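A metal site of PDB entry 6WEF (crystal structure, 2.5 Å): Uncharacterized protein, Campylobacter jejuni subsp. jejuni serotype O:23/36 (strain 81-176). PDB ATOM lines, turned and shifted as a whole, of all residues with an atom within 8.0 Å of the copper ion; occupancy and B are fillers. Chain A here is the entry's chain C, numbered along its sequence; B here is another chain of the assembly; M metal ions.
O of Leu 22 sits at hydrogen-bond distance from N of His 42, 2.8 Å away.
A ring nitrogen (ND1) of His 42 is in hydrogen-bond range of the side-chain amide oxygen (OD1) of Asn 99 (2.7 Å).
ND1 of His 95 is in hydrogen-bond range of O of Gly 93 (3.2 Å).
N of His 132 of chain B lies within hydrogen-bond range of O of Val 89, 3.0 Å away.
The backbone NH (N) of Gly 97 is in hydrogen-bond range of the backbone carbonyl oxygen (O) of Met 86 (3.0 Å).
Residues that only touch the copper ion: Gly 97.
Six residues have an atom within 4 Å of the copper ion: His 42, Glu 44, Met 88, His 95, Gly 97 and His 132 of chain B.
The nearest printed residue that does not touch the copper ion is Ala 98 (4.8 Å).
The copper ion is bound by a ring nitrogen (NE2) of His 42 (2.0 Å), a ring nitrogen (NE2) of His 95 (2.3 Å), the side-chain carboxylate (OE2) of Glu 44 (2.3 Å), a ring nitrogen (NE2) of His 132 of chain B (2.3 Å) and the side-chain sulfur (SD) of Met 88 (2.5 Å).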
ATOM      1  N   LEU A  22     -24.156 -10.498  15.879  1.00  0.00           N
ATOM      2  CA  LEU A  22     -23.850  -9.109  15.555  1.00  0.00           C
ATOM      3  C   LEU A  22     -24.633  -8.689  14.310  1.00  0.00           C
ATOM      4  O   LEU A  22     -25.502  -9.422  13.808  1.00  0.00           O
ATOM      5  CB  LEU A  22     -22.354  -8.915  15.323  1.00  0.00           C
ATOM      6  CG  LEU A  22     -21.355  -9.350  16.386  1.00  0.00           C
ATOM      7  CD1 LEU A  22     -21.073 -10.839  16.315  1.00  0.00           C
ATOM      8  CD2 LEU A  22     -20.065  -8.550  16.225  1.00  0.00           C
ATOM      9  N   GLN A  23     -24.309  -7.506  13.810  1.00  0.00           N
ATOM     10  CA  GLN A  23     -24.828  -7.058  12.519  1.00  0.00           C
ATOM     11  C   GLN A  23     -24.343  -8.010  11.418  1.00  0.00           C
ATOM     12  O   GLN A  23     -23.387  -8.755  11.612  1.00  0.00           O
ATOM     13  CB  GLN A  23     -24.349  -5.636  12.235  1.00  0.00           C
ATOM     14  CG  GLN A  23     -22.827  -5.465  12.222  1.00  0.00           C
ATOM     15  CD  GLN A  23     -22.245  -5.221  13.614  1.00  0.00           C
ATOM     16  OE1 GLN A  23     -22.893  -5.512  14.621  1.00  0.00           O
ATOM     17  NE2 GLN A  23     -21.025  -4.703  13.662  1.00  0.00           N
ATOM     18  N   ILE A  25     -22.300  -9.446   8.372  1.00  0.00           N
ATOM     19  CA  ILE A  25     -20.869  -9.342   8.185  1.00  0.00           C
ATOM     20  C   ILE A  25     -20.514  -9.699   6.751  1.00  0.00           C
ATOM     21  O   ILE A  25     -21.043 -10.661   6.190  1.00  0.00           O
ATOM     22  CB  ILE A  25     -20.101 -10.266   9.162  1.00  0.00           C
ATOM     23  CG1 ILE A  25     -20.278  -9.789  10.610  1.00  0.00           C
ATOM     24  CG2 ILE A  25     -18.638 -10.334   8.773  1.00  0.00           C
ATOM     25  CD1 ILE A  25     -19.636  -8.450  10.911  1.00  0.00           C
ATOM     26  N   MET A  27     -18.109 -11.458   4.556  1.00  0.00           N
ATOM     27  CA  MET A  27     -17.168 -12.542   4.761  1.00  0.00           C
ATOM     28  C   MET A  27     -16.649 -13.044   3.419  1.00  0.00           C
ATOM     29  O   MET A  27     -17.417 -13.219   2.472  1.00  0.00           O
ATOM     30  CB  MET A  27     -17.830 -13.704   5.519  1.00  0.00           C
ATOM     31  CG  MET A  27     -16.846 -14.680   6.132  1.00  0.00           C
ATOM     32  SD  MET A  27     -17.502 -16.358   6.267  1.00  0.00           S
ATOM     33  CE  MET A  27     -17.562 -16.847   4.545  1.00  0.00           C
ATOM     34  N   ASP A  33     -21.241 -18.045   2.183  1.00  0.00           N
ATOM     35  CA  ASP A  33     -22.302 -17.679   3.118  1.00  0.00           C
ATOM     36  C   ASP A  33     -23.199 -16.620   2.490  1.00  0.00           C
ATOM     37  O   ASP A  33     -22.825 -15.947   1.515  1.00  0.00           O
ATOM     38  CB  ASP A  33     -21.721 -17.161   4.431  1.00  0.00           C
ATOM     39  CG  ASP A  33     -22.749 -17.108   5.546  1.00  0.00           C
ATOM     40  OD1 ASP A  33     -23.763 -17.833   5.461  1.00  0.00           O
ATOM     41  OD2 ASP A  33     -22.529 -16.354   6.514  1.00  0.00           O
ATOM     42  N   HIS A  42     -25.767 -11.639  12.082  1.00  0.00           N
ATOM     43  CA  HIS A  42     -24.645 -12.562  11.917  1.00  0.00           C
ATOM     44  C   HIS A  42     -24.566 -13.406  13.181  1.00  0.00           C
ATOM     45  O   HIS A  42     -24.008 -12.968  14.195  1.00  0.00           O
ATOM     46  CB  HIS A  42     -23.336 -11.813  11.658  1.00  0.00           C
ATOM     47  CG  HIS A  42     -22.183 -12.719  11.369  1.00  0.00           C
ATOM     48  ND1 HIS A  42     -22.014 -13.337  10.155  1.00  0.00           N
ATOM     49  CD2 HIS A  42     -21.141 -13.100  12.137  1.00  0.00           C
ATOM     50  CE1 HIS A  42     -20.912 -14.078  10.185  1.00  0.00           C
ATOM     51  NE2 HIS A  42     -20.358 -13.949  11.375  1.00  0.00           N
ATOM     52  N   LEU A  43     -25.129 -14.604  13.123  1.00  0.00           N
ATOM     53  CA  LEU A  43     -25.144 -15.501  14.271  1.00  0.00           C
ATOM     54  C   LEU A  43     -23.782 -16.174  14.420  1.00  0.00           C
ATOM     55  O   LEU A  43     -23.258 -16.738  13.463  1.00  0.00           O
ATOM     56  CB  LEU A  43     -26.237 -16.548  14.106  1.00  0.00           C
ATOM     57  CG  LEU A  43     -26.436 -17.554  15.244  1.00  0.00           C
ATOM     58  CD1 LEU A  43     -26.849 -16.864  16.526  1.00  0.00           C
ATOM     59  CD2 LEU A  43     -27.457 -18.598  14.836  1.00  0.00           C
ATOM     60  N   GLU A  44     -23.227 -16.112  15.633  1.00  0.00           N
ATOM     61  CA  GLU A  44     -21.927 -16.688  15.922  1.00  0.00           C
ATOM     62  C   GLU A  44     -22.040 -17.693  17.060  1.00  0.00           C
ATOM     63  O   GLU A  44     -23.019 -17.705  17.808  1.00  0.00           O
ATOM     64  CB  GLU A  44     -20.902 -15.604  16.296  1.00  0.00           C
ATOM     65  CG  GLU A  44     -20.759 -14.509  15.253  1.00  0.00           C
ATOM     66  CD  GLU A  44     -19.356 -13.922  15.195  1.00  0.00           C
ATOM     67  OE1 GLU A  44     -18.797 -13.585  16.256  1.00  0.00           O
ATOM     68  OE2 GLU A  44     -18.802 -13.805  14.073  1.00  0.00           O
ATOM     69  N   ALA A  45     -21.031 -18.557  17.165  1.00  0.00           N
ATOM     70  CA  ALA A  45     -20.960 -19.575  18.211  1.00  0.00           C
ATOM     71  C   ALA A  45     -19.539 -19.637  18.729  1.00  0.00           C
ATOM     72  O   ALA A  45     -18.616 -19.965  17.975  1.00  0.00           O
ATOM     73  CB  ALA A  45     -21.409 -20.939  17.687  1.00  0.00           C
ATOM     74  N   MET A  86     -20.471 -21.893   9.804  1.00  0.00           N
ATOM     75  CA  MET A  86     -19.212 -22.209   9.142  1.00  0.00           C
ATOM     76  C   MET A  86     -18.035 -21.649   9.929  1.00  0.00           C
ATOM     77  O   MET A  86     -18.137 -20.580  10.541  1.00  0.00           O
ATOM     78  CB  MET A  86     -19.178 -21.649   7.720  1.00  0.00           C
ATOM     79  CG  MET A  86     -20.138 -22.322   6.732  1.00  0.00           C
ATOM     80  SD  MET A  86     -19.780 -24.057   6.374  1.00  0.00           S
ATOM     81  CE  MET A  86     -18.049 -23.984   5.918  1.00  0.00           C
ATOM     82  N   PRO A  87     -16.885 -22.332   9.924  1.00  0.00           N
ATOM     83  CA  PRO A  87     -15.710 -21.796  10.628  1.00  0.00           C
ATOM     84  C   PRO A  87     -15.153 -20.579   9.903  1.00  0.00           C
ATOM     85  O   PRO A  87     -15.127 -20.513   8.665  1.00  0.00           O
ATOM     86  CB  PRO A  87     -14.725 -22.961  10.609  1.00  0.00           C
ATOM     87  CG  PRO A  87     -15.100 -23.761   9.413  1.00  0.00           C
ATOM     88  CD  PRO A  87     -16.597 -23.620   9.277  1.00  0.00           C
ATOM     89  N   MET A  88     -14.716 -19.599  10.686  1.00  0.00           N
ATOM     90  CA  MET A  88     -14.164 -18.368  10.146  1.00  0.00           C
ATOM     91  C   MET A  88     -13.342 -17.692  11.237  1.00  0.00           C
ATOM     92  O   MET A  88     -13.137 -18.260  12.310  1.00  0.00           O
ATOM     93  CB  MET A  88     -15.283 -17.455   9.635  1.00  0.00           C
ATOM     94  CG  MET A  88     -16.109 -16.800  10.724  1.00  0.00           C
ATOM     95  SD  MET A  88     -17.535 -15.926  10.050  1.00  0.00           S
ATOM     96  CE  MET A  88     -18.528 -17.294   9.447  1.00  0.00           C
ATOM     97  N   VAL A  89     -12.864 -16.488  10.960  1.00  0.00           N
ATOM     98  CA  VAL A  89     -12.043 -15.737  11.898  1.00  0.00           C
ATOM     99  C   VAL A  89     -12.340 -14.262  11.717  1.00  0.00           C
ATOM    100  O   VAL A  89     -12.543 -13.780  10.597  1.00  0.00           O
ATOM    101  CB  VAL A  89     -10.541 -16.033  11.703  1.00  0.00           C
ATOM    102  CG1 VAL A  89     -10.106 -15.668  10.282  1.00  0.00           C
ATOM    103  CG2 VAL A  89      -9.708 -15.286  12.728  1.00  0.00           C
ATOM    104  N   ALA A  90     -12.361 -13.541  12.840  1.00  0.00           N
ATOM    105  CA  ALA A  90     -12.485 -12.086  12.858  1.00  0.00           C
ATOM    106  C   ALA A  90     -11.313 -11.508  13.661  1.00  0.00           C
ATOM    107  O   ALA A  90     -10.339 -12.206  13.956  1.00  0.00           O
ATOM    108  CB  ALA A  90     -13.839 -11.673  13.445  1.00  0.00           C
ATOM    109  N   GLY A  93     -10.496 -13.631  16.911  1.00  0.00           N
ATOM    110  CA  GLY A  93     -10.203 -15.042  16.913  1.00  0.00           C
ATOM    111  C   GLY A  93     -11.158 -15.866  16.081  1.00  0.00           C
ATOM    112  O   GLY A  93     -12.203 -15.385  15.639  1.00  0.00           O
ATOM    113  N   PRO A  94     -10.817 -17.134  15.865  1.00  0.00           N
ATOM    114  CA  PRO A  94     -11.684 -18.008  15.064  1.00  0.00           C
ATOM    115  C   PRO A  94     -12.985 -18.310  15.785  1.00  0.00           C
ATOM    116  O   PRO A  94     -13.097 -18.200  17.004  1.00  0.00           O
ATOM    117  CB  PRO A  94     -10.834 -19.282  14.891  1.00  0.00           C
ATOM    118  CG  PRO A  94      -9.920 -19.292  16.072  1.00  0.00           C
ATOM    119  CD  PRO A  94      -9.624 -17.837  16.376  1.00  0.00           C
ATOM    120  N   HIS A  95     -13.977 -18.705  14.990  1.00  0.00           N
ATOM    121  CA  HIS A  95     -15.306 -18.987  15.517  1.00  0.00           C
ATOM    122  C   HIS A  95     -16.137 -19.599  14.397  1.00  0.00           C
ATOM    123  O   HIS A  95     -15.674 -19.745  13.257  1.00  0.00           O
ATOM    124  CB  HIS A  95     -15.964 -17.714  16.050  1.00  0.00           C
ATOM    125  CG  HIS A  95     -16.196 -16.665  15.003  1.00  0.00           C
ATOM    126  ND1 HIS A  95     -15.258 -15.709  14.685  1.00  0.00           N
ATOM    127  CD2 HIS A  95     -17.259 -16.431  14.205  1.00  0.00           C
ATOM    128  CE1 HIS A  95     -15.737 -14.927  13.738  1.00  0.00           C
ATOM    129  NE2 HIS A  95     -16.946 -15.343  13.419  1.00  0.00           N
ATOM    130  N   TYR A  96     -17.365 -19.962  14.730  1.00  0.00           N
ATOM    131  CA  TYR A  96     -18.357 -20.450  13.772  1.00  0.00           C
ATOM    132  C   TYR A  96     -19.457 -19.405  13.655  1.00  0.00           C
ATOM    133  O   TYR A  96     -20.063 -19.019  14.662  1.00  0.00           O
ATOM    134  CB  TYR A  96     -18.939 -21.786  14.209  1.00  0.00           C
ATOM    135  CG  TYR A  96     -17.903 -22.860  14.455  1.00  0.00           C
ATOM    136  CD1 TYR A  96     -17.302 -22.996  15.704  1.00  0.00           C
ATOM    137  CD2 TYR A  96     -17.538 -23.754  13.451  1.00  0.00           C
ATOM    138  CE1 TYR A  96     -16.360 -23.978  15.940  1.00  0.00           C
ATOM    139  CE2 TYR A  96     -16.605 -24.740  13.682  1.00  0.00           C
ATOM    140  CZ  TYR A  96     -16.012 -24.846  14.927  1.00  0.00           C
ATOM    141  OH  TYR A  96     -15.071 -25.828  15.163  1.00  0.00           O
ATOM    142  N   GLY A  97     -19.731 -18.958  12.430  1.00  0.00           N
ATOM    143  CA  GLY A  97     -20.734 -17.928  12.222  1.00  0.00           C
ATOM    144  C   GLY A  97     -21.482 -18.113  10.920  1.00  0.00           C
ATOM    145  O   GLY A  97     -21.157 -18.983  10.110  1.00  0.00           O
ATOM    146  N   ALA A  98     -22.492 -17.274  10.732  1.00  0.00           N
ATOM    147  CA  ALA A  98     -23.307 -17.316   9.526  1.00  0.00           C
ATOM    148  C   ALA A  98     -24.216 -16.101   9.507  1.00  0.00           C
ATOM    149  O   ALA A  98     -24.722 -15.674  10.549  1.00  0.00           O
ATOM    150  CB  ALA A  98     -24.142 -18.600   9.463  1.00  0.00           C
ATOM    151  N   ASN A  99     -24.425 -15.546   8.307  1.00  0.00           N
ATOM    152  CA  ASN A  99     -25.365 -14.462   8.102  1.00  0.00           C
ATOM    153  C   ASN A  99     -26.751 -15.044   7.862  1.00  0.00           C
ATOM    154  O   ASN A  99     -26.909 -15.965   7.047  1.00  0.00           O
ATOM    155  CB  ASN A  99     -24.950 -13.586   6.922  1.00  0.00           C
ATOM    156  CG  ASN A  99     -23.766 -12.689   7.242  1.00  0.00           C
ATOM    157  OD1 ASN A  99     -23.634 -12.205   8.376  1.00  0.00           O
ATOM    158  ND2 ASN A  99     -22.898 -12.463   6.265  1.00  0.00           N
ATOM    159  N   GLY B 130     -13.728 -19.092   6.693  1.00  0.00           N
ATOM    160  CA  GLY B 130     -14.192 -17.743   6.483  1.00  0.00           C
ATOM    161  C   GLY B 130     -13.249 -16.690   7.036  1.00  0.00           C
ATOM    162  O   GLY B 130     -12.333 -16.964   7.817  1.00  0.00           O
ATOM    163  N   ARG B 131     -13.516 -15.451   6.635  1.00  0.00           N
ATOM    164  CA  ARG B 131     -12.714 -14.312   7.056  1.00  0.00           C
ATOM    165  C   ARG B 131     -13.579 -13.071   7.009  1.00  0.00           C
ATOM    166  O   ARG B 131     -14.031 -12.666   5.923  1.00  0.00           O
ATOM    167  CB  ARG B 131     -11.484 -14.161   6.165  1.00  0.00           C
ATOM    168  CG  ARG B 131     -10.722 -12.866   6.402  1.00  0.00           C
ATOM    169  CD  ARG B 131      -9.372 -12.866   5.702  1.00  0.00           C
ATOM    170  NE  ARG B 131      -9.508 -12.776   4.246  1.00  0.00           N
ATOM    171  CZ  ARG B 131      -9.490 -11.647   3.550  1.00  0.00           C
ATOM    172  NH1 ARG B 131      -9.332 -10.477   4.155  1.00  0.00           N
ATOM    173  NH2 ARG B 131      -9.634 -11.683   2.234  1.00  0.00           N
ATOM    174  N   HIS B 132     -13.824 -12.464   8.172  1.00  0.00           N
ATOM    175  CA  HIS B 132     -14.521 -11.183   8.210  1.00  0.00           C
ATOM    176  C   HIS B 132     -13.714 -10.125   7.465  1.00  0.00           C
ATOM    177  O   HIS B 132     -12.519  -9.948   7.724  1.00  0.00           O
ATOM    178  CB  HIS B 132     -14.747 -10.744   9.661  1.00  0.00           C
ATOM    179  CG  HIS B 132     -15.792 -11.541  10.375  1.00  0.00           C
ATOM    180  ND1 HIS B 132     -16.508 -11.025  11.438  1.00  0.00           N
ATOM    181  CD2 HIS B 132     -16.240 -12.800  10.190  1.00  0.00           C
ATOM    182  CE1 HIS B 132     -17.359 -11.940  11.871  1.00  0.00           C
ATOM    183  NE2 HIS B 132     -17.210 -13.025  11.131  1.00  0.00           N
ATOM    184  N   ASP B 134     -15.305  -6.966   7.032  1.00  0.00           N
ATOM    185  CA  ASP B 134     -15.996  -5.723   7.332  1.00  0.00           C
ATOM    186  C   ASP B 134     -15.026  -4.722   7.936  1.00  0.00           C
ATOM    187  O   ASP B 134     -13.951  -5.069   8.421  1.00  0.00           O
ATOM    188  CB  ASP B 134     -17.174  -5.964   8.279  1.00  0.00           C
ATOM    189  CG  ASP B 134     -16.775  -6.693   9.549  1.00  0.00           C
ATOM    190  OD1 ASP B 134     -16.320  -7.846   9.456  1.00  0.00           O
ATOM    191  OD2 ASP B 134     -16.930  -6.114  10.644  1.00  0.00           O
ATOM    192  N   THR B 137     -14.869  -5.294  12.231  1.00  0.00           N
ATOM    193  CA  THR B 137     -14.422  -6.555  12.799  1.00  0.00           C
ATOM    194  C   THR B 137     -13.660  -7.423  11.797  1.00  0.00           C
ATOM    195  O   THR B 137     -13.587  -8.637  11.969  1.00  0.00           O
ATOM    196  CB  THR B 137     -15.616  -7.332  13.357  1.00  0.00           C
HETATM  197 CU    CU M   1     -18.586 -14.732  11.966  1.00  0.00          CU
